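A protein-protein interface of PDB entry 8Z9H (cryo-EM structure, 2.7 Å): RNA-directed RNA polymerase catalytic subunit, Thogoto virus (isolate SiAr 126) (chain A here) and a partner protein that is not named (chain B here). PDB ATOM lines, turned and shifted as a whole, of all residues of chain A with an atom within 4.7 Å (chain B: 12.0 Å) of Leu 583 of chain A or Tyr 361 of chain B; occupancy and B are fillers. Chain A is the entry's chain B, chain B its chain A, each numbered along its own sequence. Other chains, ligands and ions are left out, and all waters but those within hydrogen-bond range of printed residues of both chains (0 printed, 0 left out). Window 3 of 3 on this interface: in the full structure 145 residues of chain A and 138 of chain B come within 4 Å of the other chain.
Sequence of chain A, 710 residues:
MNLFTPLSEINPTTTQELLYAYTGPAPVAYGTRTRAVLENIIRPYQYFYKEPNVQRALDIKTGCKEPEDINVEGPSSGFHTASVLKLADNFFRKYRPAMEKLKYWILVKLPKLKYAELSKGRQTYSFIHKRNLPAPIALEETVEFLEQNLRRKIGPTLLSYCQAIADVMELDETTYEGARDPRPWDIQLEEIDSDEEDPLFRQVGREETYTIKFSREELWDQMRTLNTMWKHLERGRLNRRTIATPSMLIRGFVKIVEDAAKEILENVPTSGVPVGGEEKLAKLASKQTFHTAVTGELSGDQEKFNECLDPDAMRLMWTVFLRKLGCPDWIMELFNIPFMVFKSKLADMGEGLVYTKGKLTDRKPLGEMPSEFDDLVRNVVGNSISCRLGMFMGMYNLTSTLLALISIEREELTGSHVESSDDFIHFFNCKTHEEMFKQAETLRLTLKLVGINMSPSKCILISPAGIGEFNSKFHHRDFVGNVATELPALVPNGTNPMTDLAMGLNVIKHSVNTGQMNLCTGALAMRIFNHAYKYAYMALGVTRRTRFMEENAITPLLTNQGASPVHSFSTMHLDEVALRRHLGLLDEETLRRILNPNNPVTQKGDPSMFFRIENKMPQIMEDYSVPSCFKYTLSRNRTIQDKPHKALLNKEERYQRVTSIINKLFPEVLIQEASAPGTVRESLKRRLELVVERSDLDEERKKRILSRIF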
ATOM      1  N   VAL A 566     -30.561  -9.334   4.098  1.00  0.00           N
ATOM      2  CA  VAL A 566     -29.449  -8.557   3.566  1.00  0.00           C
ATOM      3  C   VAL A 566     -29.731  -7.060   3.627  1.00  0.00           C
ATOM      4  O   VAL A 566     -28.780  -6.264   3.686  1.00  0.00           O
ATOM      5  CB  VAL A 566     -29.119  -8.991   2.121  1.00  0.00           C
ATOM      6  CG1 VAL A 566     -30.241  -8.604   1.168  1.00  0.00           C
ATOM      7  CG2 VAL A 566     -27.785  -8.415   1.667  1.00  0.00           C
ATOM      8  N   SER A 568     -30.478  -3.615   5.272  1.00  0.00           N
ATOM      9  CA  SER A 568     -30.299  -2.934   6.541  1.00  0.00           C
ATOM     10  C   SER A 568     -31.152  -1.671   6.547  1.00  0.00           C
ATOM     11  O   SER A 568     -31.916  -1.407   5.616  1.00  0.00           O
ATOM     12  CB  SER A 568     -28.824  -2.616   6.771  1.00  0.00           C
ATOM     13  OG  SER A 568     -28.660  -1.834   7.935  1.00  0.00           O
ATOM     14  N   THR A 571     -29.923   0.421   3.746  1.00  0.00           N
ATOM     15  CA  THR A 571     -30.046  -0.228   2.446  1.00  0.00           C
ATOM     16  C   THR A 571     -31.505  -0.510   2.098  1.00  0.00           C
ATOM     17  O   THR A 571     -31.831  -1.535   1.501  1.00  0.00           O
ATOM     18  CB  THR A 571     -29.231  -1.517   2.405  1.00  0.00           C
ATOM     19  OG1 THR A 571     -29.734  -2.433   3.383  1.00  0.00           O
ATOM     20  CG2 THR A 571     -27.771  -1.228   2.703  1.00  0.00           C
ATOM     21  N   LEU A 579     -27.339  -6.239  -4.099  1.00  0.00           N
ATOM     22  CA  LEU A 579     -26.629  -6.080  -2.834  1.00  0.00           C
ATOM     23  C   LEU A 579     -25.975  -7.384  -2.395  1.00  0.00           C
ATOM     24  O   LEU A 579     -24.835  -7.384  -1.915  1.00  0.00           O
ATOM     25  CB  LEU A 579     -27.586  -5.566  -1.760  1.00  0.00           C
ATOM     26  CG  LEU A 579     -27.004  -5.369  -0.361  1.00  0.00           C
ATOM     27  CD1 LEU A 579     -25.818  -4.425  -0.411  1.00  0.00           C
ATOM     28  CD2 LEU A 579     -28.068  -4.844   0.585  1.00  0.00           C
ATOM     29  N   ARG A 580     -26.679  -8.508  -2.551  1.00  0.00           N
ATOM     30  CA  ARG A 580     -26.097  -9.799  -2.197  1.00  0.00           C
ATOM     31  C   ARG A 580     -24.907 -10.128  -3.088  1.00  0.00           C
ATOM     32  O   ARG A 580     -23.906 -10.681  -2.618  1.00  0.00           O
ATOM     33  CB  ARG A 580     -27.154 -10.899  -2.283  1.00  0.00           C
ATOM     34  CG  ARG A 580     -28.235 -10.795  -1.226  1.00  0.00           C
ATOM     35  CD  ARG A 580     -29.096 -12.043  -1.180  1.00  0.00           C
ATOM     36  NE  ARG A 580     -30.027 -12.011  -0.059  1.00  0.00           N
ATOM     37  CZ  ARG A 580     -29.720 -12.372   1.179  1.00  0.00           C
ATOM     38  NH1 ARG A 580     -28.512 -12.809   1.493  1.00  0.00           N
ATOM     39  NH2 ARG A 580     -30.649 -12.291   2.127  1.00  0.00           N
ATOM     40  N   ARG A 581     -25.000  -9.804  -4.380  1.00  0.00           N
ATOM     41  CA  ARG A 581     -23.866 -10.014  -5.271  1.00  0.00           C
ATOM     42  C   ARG A 581     -22.677  -9.155  -4.860  1.00  0.00           C
ATOM     43  O   ARG A 581     -21.532  -9.621  -4.869  1.00  0.00           O
ATOM     44  CB  ARG A 581     -24.269  -9.713  -6.713  1.00  0.00           C
ATOM     45  CG  ARG A 581     -23.108  -9.731  -7.690  1.00  0.00           C
ATOM     46  CD  ARG A 581     -23.445  -8.985  -8.964  1.00  0.00           C
ATOM     47  NE  ARG A 581     -22.670  -9.477 -10.095  1.00  0.00           N
ATOM     48  CZ  ARG A 581     -22.665  -8.921 -11.299  1.00  0.00           C
ATOM     49  NH1 ARG A 581     -23.383  -7.841 -11.563  1.00  0.00           N
ATOM     50  NH2 ARG A 581     -21.924  -9.462 -12.261  1.00  0.00           N
ATOM     51  N   HIS A 582     -22.932  -7.896  -4.502  1.00  0.00           N
ATOM     52  CA  HIS A 582     -21.849  -7.006  -4.099  1.00  0.00           C
ATOM     53  C   HIS A 582     -21.184  -7.485  -2.815  1.00  0.00           C
ATOM     54  O   HIS A 582     -19.957  -7.422  -2.683  1.00  0.00           O
ATOM     55  CB  HIS A 582     -22.377  -5.584  -3.931  1.00  0.00           C
ATOM     56  CG  HIS A 582     -21.368  -4.624  -3.383  1.00  0.00           C
ATOM     57  ND1 HIS A 582     -20.459  -3.966  -4.181  1.00  0.00           N
ATOM     58  CD2 HIS A 582     -21.129  -4.208  -2.117  1.00  0.00           C
ATOM     59  CE1 HIS A 582     -19.700  -3.188  -3.431  1.00  0.00           C
ATOM     60  NE2 HIS A 582     -20.086  -3.316  -2.175  1.00  0.00           N
ATOM     61  N   LEU A 583     -21.976  -7.969  -1.858  1.00  0.00           N
ATOM     62  CA  LEU A 583     -21.429  -8.435  -0.591  1.00  0.00           C
ATOM     63  C   LEU A 583     -20.857  -9.842  -0.667  1.00  0.00           C
ATOM     64  O   LEU A 583     -20.279 -10.310   0.320  1.00  0.00           O
ATOM     65  CB  LEU A 583     -22.503  -8.381   0.498  1.00  0.00           C
ATOM     66  CG  LEU A 583     -22.967  -6.986   0.911  1.00  0.00           C
ATOM     67  CD1 LEU A 583     -24.087  -7.083   1.927  1.00  0.00           C
ATOM     68  CD2 LEU A 583     -21.806  -6.182   1.464  1.00  0.00           C
ATOM     69  N   GLY A 584     -21.002 -10.527  -1.798  1.00  0.00           N
ATOM     70  CA  GLY A 584     -20.494 -11.872  -1.941  1.00  0.00           C
ATOM     71  C   GLY A 584     -21.390 -12.959  -1.395  1.00  0.00           C
ATOM     72  O   GLY A 584     -21.004 -14.134  -1.434  1.00  0.00           O
ATOM     73  N   LEU A 585     -22.572 -12.612  -0.884  1.00  0.00           N
ATOM     74  CA  LEU A 585     -23.499 -13.609  -0.368  1.00  0.00           C
ATOM     75  C   LEU A 585     -24.167 -14.418  -1.470  1.00  0.00           C
ATOM     76  O   LEU A 585     -24.822 -15.421  -1.168  1.00  0.00           O
ATOM     77  CB  LEU A 585     -24.568 -12.932   0.491  1.00  0.00           C
ATOM     78  CG  LEU A 585     -24.056 -12.062   1.638  1.00  0.00           C
ATOM     79  CD1 LEU A 585     -25.168 -11.180   2.176  1.00  0.00           C
ATOM     80  CD2 LEU A 585     -23.472 -12.927   2.740  1.00  0.00           C
ATOM     81  N   GLU B 356     -36.005 -11.795  13.455  1.00  0.00           N
ATOM     82  CA  GLU B 356     -34.661 -11.863  12.901  1.00  0.00           C
ATOM     83  C   GLU B 356     -34.060 -10.468  12.805  1.00  0.00           C
ATOM     84  O   GLU B 356     -34.694  -9.538  12.299  1.00  0.00           O
ATOM     85  CB  GLU B 356     -34.694 -12.525  11.525  1.00  0.00           C
ATOM     86  CG  GLU B 356     -33.378 -13.148  11.101  1.00  0.00           C
ATOM     87  CD  GLU B 356     -33.546 -14.135   9.964  1.00  0.00           C
ATOM     88  OE1 GLU B 356     -34.665 -14.222   9.415  1.00  0.00           O
ATOM     89  OE2 GLU B 356     -32.563 -14.822   9.620  1.00  0.00           O
ATOM     90  N   LYS B 357     -32.835 -10.324  13.298  1.00  0.00           N
ATOM     91  CA  LYS B 357     -32.183  -9.025  13.304  1.00  0.00           C
ATOM     92  C   LYS B 357     -31.803  -8.612  11.889  1.00  0.00           C
ATOM     93  O   LYS B 357     -31.334  -9.428  11.090  1.00  0.00           O
ATOM     94  CB  LYS B 357     -30.940  -9.058  14.193  1.00  0.00           C
ATOM     95  CG  LYS B 357     -31.237  -9.322  15.658  1.00  0.00           C
ATOM     96  CD  LYS B 357     -29.972  -9.283  16.496  1.00  0.00           C
ATOM     97  CE  LYS B 357     -30.253  -9.699  17.930  1.00  0.00           C
ATOM     98  NZ  LYS B 357     -31.132  -8.726  18.631  1.00  0.00           N
ATOM     99  N   ASN B 358     -32.010  -7.337  11.580  1.00  0.00           N
ATOM    100  CA  ASN B 358     -31.609  -6.812  10.287  1.00  0.00           C
ATOM    101  C   ASN B 358     -30.088  -6.727  10.199  1.00  0.00           C
ATOM    102  O   ASN B 358     -29.377  -6.753  11.206  1.00  0.00           O
ATOM    103  CB  ASN B 358     -32.222  -5.433  10.051  1.00  0.00           C
ATOM    104  CG  ASN B 358     -33.718  -5.488   9.832  1.00  0.00           C
ATOM    105  OD1 ASN B 358     -34.264  -6.531   9.480  1.00  0.00           O
ATOM    106  ND2 ASN B 358     -34.390  -4.363  10.045  1.00  0.00           N
ATOM    107  N   ALA B 359     -29.594  -6.631   8.969  1.00  0.00           N
ATOM    108  CA  ALA B 359     -28.164  -6.482   8.754  1.00  0.00           C
ATOM    109  C   ALA B 359     -27.679  -5.150   9.314  1.00  0.00           C
ATOM    110  O   ALA B 359     -28.439  -4.187   9.438  1.00  0.00           O
ATOM    111  CB  ALA B 359     -27.834  -6.578   7.266  1.00  0.00           C
ATOM    112  N   ILE B 360     -26.402  -5.109   9.679  1.00  0.00           N
ATOM    113  CA  ILE B 360     -25.770  -3.906  10.206  1.00  0.00           C
ATOM    114  C   ILE B 360     -24.550  -3.605   9.350  1.00  0.00           C
ATOM    115  O   ILE B 360     -23.620  -4.418   9.276  1.00  0.00           O
ATOM    116  CB  ILE B 360     -25.380  -4.065  11.682  1.00  0.00           C
ATOM    117  CG1 ILE B 360     -26.632  -4.218  12.547  1.00  0.00           C
ATOM    118  CG2 ILE B 360     -24.553  -2.877  12.145  1.00  0.00           C
ATOM    119  CD1 ILE B 360     -26.341  -4.564  13.987  1.00  0.00           C
ATOM    120  N   TYR B 361     -24.553  -2.444   8.708  1.00  0.00           N
ATOM    121  CA  TYR B 361     -23.442  -2.005   7.875  1.00  0.00           C
ATOM    122  C   TYR B 361     -22.845  -0.685   8.329  1.00  0.00           C
ATOM    123  O   TYR B 361     -21.622  -0.528   8.311  1.00  0.00           O
ATOM    124  CB  TYR B 361     -23.892  -1.879   6.412  1.00  0.00           C
ATOM    125  CG  TYR B 361     -24.514  -3.135   5.849  1.00  0.00           C
ATOM    126  CD1 TYR B 361     -23.941  -4.379   6.072  1.00  0.00           C
ATOM    127  CD2 TYR B 361     -25.676  -3.077   5.096  1.00  0.00           C
ATOM    128  CE1 TYR B 361     -24.509  -5.528   5.559  1.00  0.00           C
ATOM    129  CE2 TYR B 361     -26.251  -4.220   4.580  1.00  0.00           C
ATOM    130  CZ  TYR B 361     -25.663  -5.441   4.815  1.00  0.00           C
ATOM    131  OH  TYR B 361     -26.234  -6.583   4.303  1.00  0.00           O
ATOM    132  N   THR B 362     -23.675   0.268   8.740  1.00  0.00           N
ATOM    133  CA  THR B 362     -23.227   1.581   9.172  1.00  0.00           C
ATOM    134  C   THR B 362     -23.527   1.779  10.653  1.00  0.00           C
ATOM    135  O   THR B 362     -24.217   0.979  11.289  1.00  0.00           O
ATOM    136  CB  THR B 362     -23.894   2.684   8.344  1.00  0.00           C
ATOM    137  OG1 THR B 362     -25.220   2.915   8.835  1.00  0.00           O
ATOM    138  CG2 THR B 362     -23.970   2.281   6.882  1.00  0.00           C
ATOM    139  N   GLU B 363     -22.985   2.868  11.198  1.00  0.00           N
ATOM    140  CA  GLU B 363     -23.224   3.198  12.599  1.00  0.00           C
ATOM    141  C   GLU B 363     -24.670   3.619  12.840  1.00  0.00           C
ATOM    142  O   GLU B 363     -25.212   3.379  13.926  1.00  0.00           O
ATOM    143  CB  GLU B 363     -22.251   4.290  13.046  1.00  0.00           C
ATOM    144  CG  GLU B 363     -22.399   5.605  12.300  1.00  0.00           C
ATOM    145  CD  GLU B 363     -21.645   5.629  10.982  1.00  0.00           C
ATOM    146  OE1 GLU B 363     -21.202   4.556  10.521  1.00  0.00           O
ATOM    147  OE2 GLU B 363     -21.503   6.725  10.402  1.00  0.00           O
ATOM    148  N   VAL B 364     -25.307   4.244  11.846  1.00  0.00           N
ATOM    149  CA  VAL B 364     -26.737   4.525  11.937  1.00  0.00           C
ATOM    150  C   VAL B 364     -27.518   3.227  12.062  1.00  0.00           C
ATOM    151  O   VAL B 364     -28.441   3.109  12.880  1.00  0.00           O
ATOM    152  CB  VAL B 364     -27.195   5.345  10.717  1.00  0.00           C
ATOM    153  CG1 VAL B 364     -28.703   5.491  10.711  1.00  0.00           C
ATOM    154  CG2 VAL B 364     -26.529   6.708  10.712  1.00  0.00           C
ATOM    155  N   ASP B 365     -27.152   2.228  11.259  1.00  0.00           N
ATOM    156  CA  ASP B 365     -27.775   0.917  11.377  1.00  0.00           C
ATOM    157  C   ASP B 365     -27.523   0.320  12.753  1.00  0.00           C
ATOM    158  O   ASP B 365     -28.419  -0.290  13.348  1.00  0.00           O
ATOM    159  CB  ASP B 365     -27.243  -0.006  10.285  1.00  0.00           C
ATOM    160  CG  ASP B 365     -27.434   0.566   8.897  1.00  0.00           C
ATOM    161  OD1 ASP B 365     -28.363   1.377   8.709  1.00  0.00           O
ATOM    162  OD2 ASP B 365     -26.660   0.199   7.990  1.00  0.00           O
ATOM    163  N   GLY B 366     -26.308   0.491  13.275  1.00  0.00           N
ATOM    164  CA  GLY B 366     -25.999  -0.040  14.592  1.00  0.00           C
ATOM    165  C   GLY B 366     -26.865   0.559  15.683  1.00  0.00           C
ATOM    166  O   GLY B 366     -27.410  -0.161  16.522  1.00  0.00           O
ATOM    167  N   VAL B 367     -27.016   1.885  15.681  1.00  0.00           N
ATOM    168  CA  VAL B 367     -27.827   2.521  16.715  1.00  0.00           C
ATOM    169  C   VAL B 367     -29.301   2.171  16.534  1.00  0.00           C
ATOM    170  O   VAL B 367     -30.032   1.994  17.518  1.00  0.00           O
ATOM    171  CB  VAL B 367     -27.590   4.045  16.748  1.00  0.00           C
ATOM    172  CG1 VAL B 367     -26.125   4.347  17.023  1.00  0.00           C
ATOM    173  CG2 VAL B 367     -28.038   4.709  15.464  1.00  0.00           C
ATOM    174  N   ALA B 368     -29.760   2.047  15.285  1.00  0.00           N
ATOM    175  CA  ALA B 368     -31.148   1.661  15.050  1.00  0.00           C
ATOM    176  C   ALA B 368     -31.431   0.268  15.600  1.00  0.00           C
ATOM    177  O   ALA B 368     -32.431   0.051  16.299  1.00  0.00           O
ATOM    178  CB  ALA B 368     -31.465   1.728  13.556  1.00  0.00           C
ATOM    179  N   GLU B 369     -30.551  -0.693  15.307  1.00  0.00           N
ATOM    180  CA  GLU B 369     -30.760  -2.042  15.819  1.00  0.00           C
ATOM    181  C   GLU B 369     -30.578  -2.106  17.329  1.00  0.00           C
ATOM    182  O   GLU B 369     -31.240  -2.910  17.990  1.00  0.00           O
ATOM    183  CB  GLU B 369     -29.835  -3.037  15.121  1.00  0.00           C
ATOM    184  CG  GLU B 369     -29.864  -2.940  13.610  1.00  0.00           C
ATOM    185  CD  GLU B 369     -31.177  -3.409  13.019  1.00  0.00           C
ATOM    186  OE1 GLU B 369     -31.880  -4.205  13.675  1.00  0.00           O
ATOM    187  OE2 GLU B 369     -31.513  -2.966  11.901  1.00  0.00           O
ATOM    188  N   GLY B 370     -29.704  -1.272  17.895  1.00  0.00           N
ATOM    189  CA  GLY B 370     -29.603  -1.211  19.344  1.00  0.00           C
ATOM    190  C   GLY B 370     -30.885  -0.725  19.993  1.00  0.00           C
ATOM    191  O   GLY B 370     -31.338  -1.286  20.995  1.00  0.00           O
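Of the 10 printed residues of chain A, 4 touch a printed residue of chain B.
Hydrophobic or aromatic side chains of chain A that line the printed part of chain B: Val 566 and Leu 583.
Printed residues of chain B that touch a printed residue of chain A: Ala 359, Tyr 361 and Asp 365.
Hydrophobic or aromatic side chains of chain B that line the printed part of chain A: Ala 359 and Tyr 361.
Among the printed residues, 7 pairs touch across the chains.
Among the printed residues, no Asp or Glu carboxylate lies within 4 Å of a Lys or Arg side-chain nitrogen of the other chain.
Val 566 of chain A touches two residues of chain B.
Of chain B, only Ala 359, Tyr 361 and Asp 365 come within 4 Å of Ser 568 of chain A.
Of chain B, only Tyr 361 comes within 4 Å of Thr 571 of chain A.
No residue of chain B comes within 4 Å of Arg 580 of chain A.
No residue of chain B comes within 4 Å of His 582 of chain A.
Leu 583 of chain A touches just one residue of chain B: Tyr 361 (3.2 Å).
No residue of chain B comes within 4 Å of Gly 584 of chain A.
No residue of chain B comes within 4 Å of Leu 585 of chain A.
Of the printed residues of chain A, Ala 359 of chain B touches Val 566 and Ser 568.
Of chain A, only Val 566, Ser 568, Thr 571 and Leu 583 come within 4 Å of Tyr 361 of chain B.
Of the printed residues of chain A, Asp 365 of chain B touches Ser 568 (2.9 Å).
The nearest residue of chain B that does not touch Leu 583 of chain A is Ala 359 of chain B (6.5 Å).
The side-chain hydroxyl of Ser 568 of chain A sits at hydrogen-bond distance from the backbone carbonyl oxygen of Ala 359 of chain B (2.8 Å).
The side-chain hydroxyl of Tyr 361 of chain B lies within hydrogen-bond range of the backbone carbonyl oxygen of Val 566 of chain A (2.6 Å).
The side-chain carboxylate of Asp 365 of chain B is in hydrogen-bond range of the side-chain hydroxyl of Ser 568 of chain A, at 2.9 Å.
Val 566 of chain A touches Ala 359 of chain B (O to CB, 3.7 Å).
CB of Ser 568 of chain A touches CD2 of Tyr 361 of chain B, 3.6 Å away.
Thr 571 of chain A touches Tyr 361 of chain B (CG2 to CD2, 3.7 Å).
OH of Tyr 361 of chain B touches CD1 of Leu 583 of chain A, 3.2 Å away.
N of Tyr 361 of chain B lies within hydrogen-bond range of OD2 of Asp 365 of chain B, 3.5 Å away.
OD2 of Asp 365 of chain B is in hydrogen-bond range of N of Thr 362 of chain B (3.1 Å).
The side-chain hydroxyl of Thr 571 of chain A sits close to the backbone carbonyl oxygen of Ser 568 of chain A.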
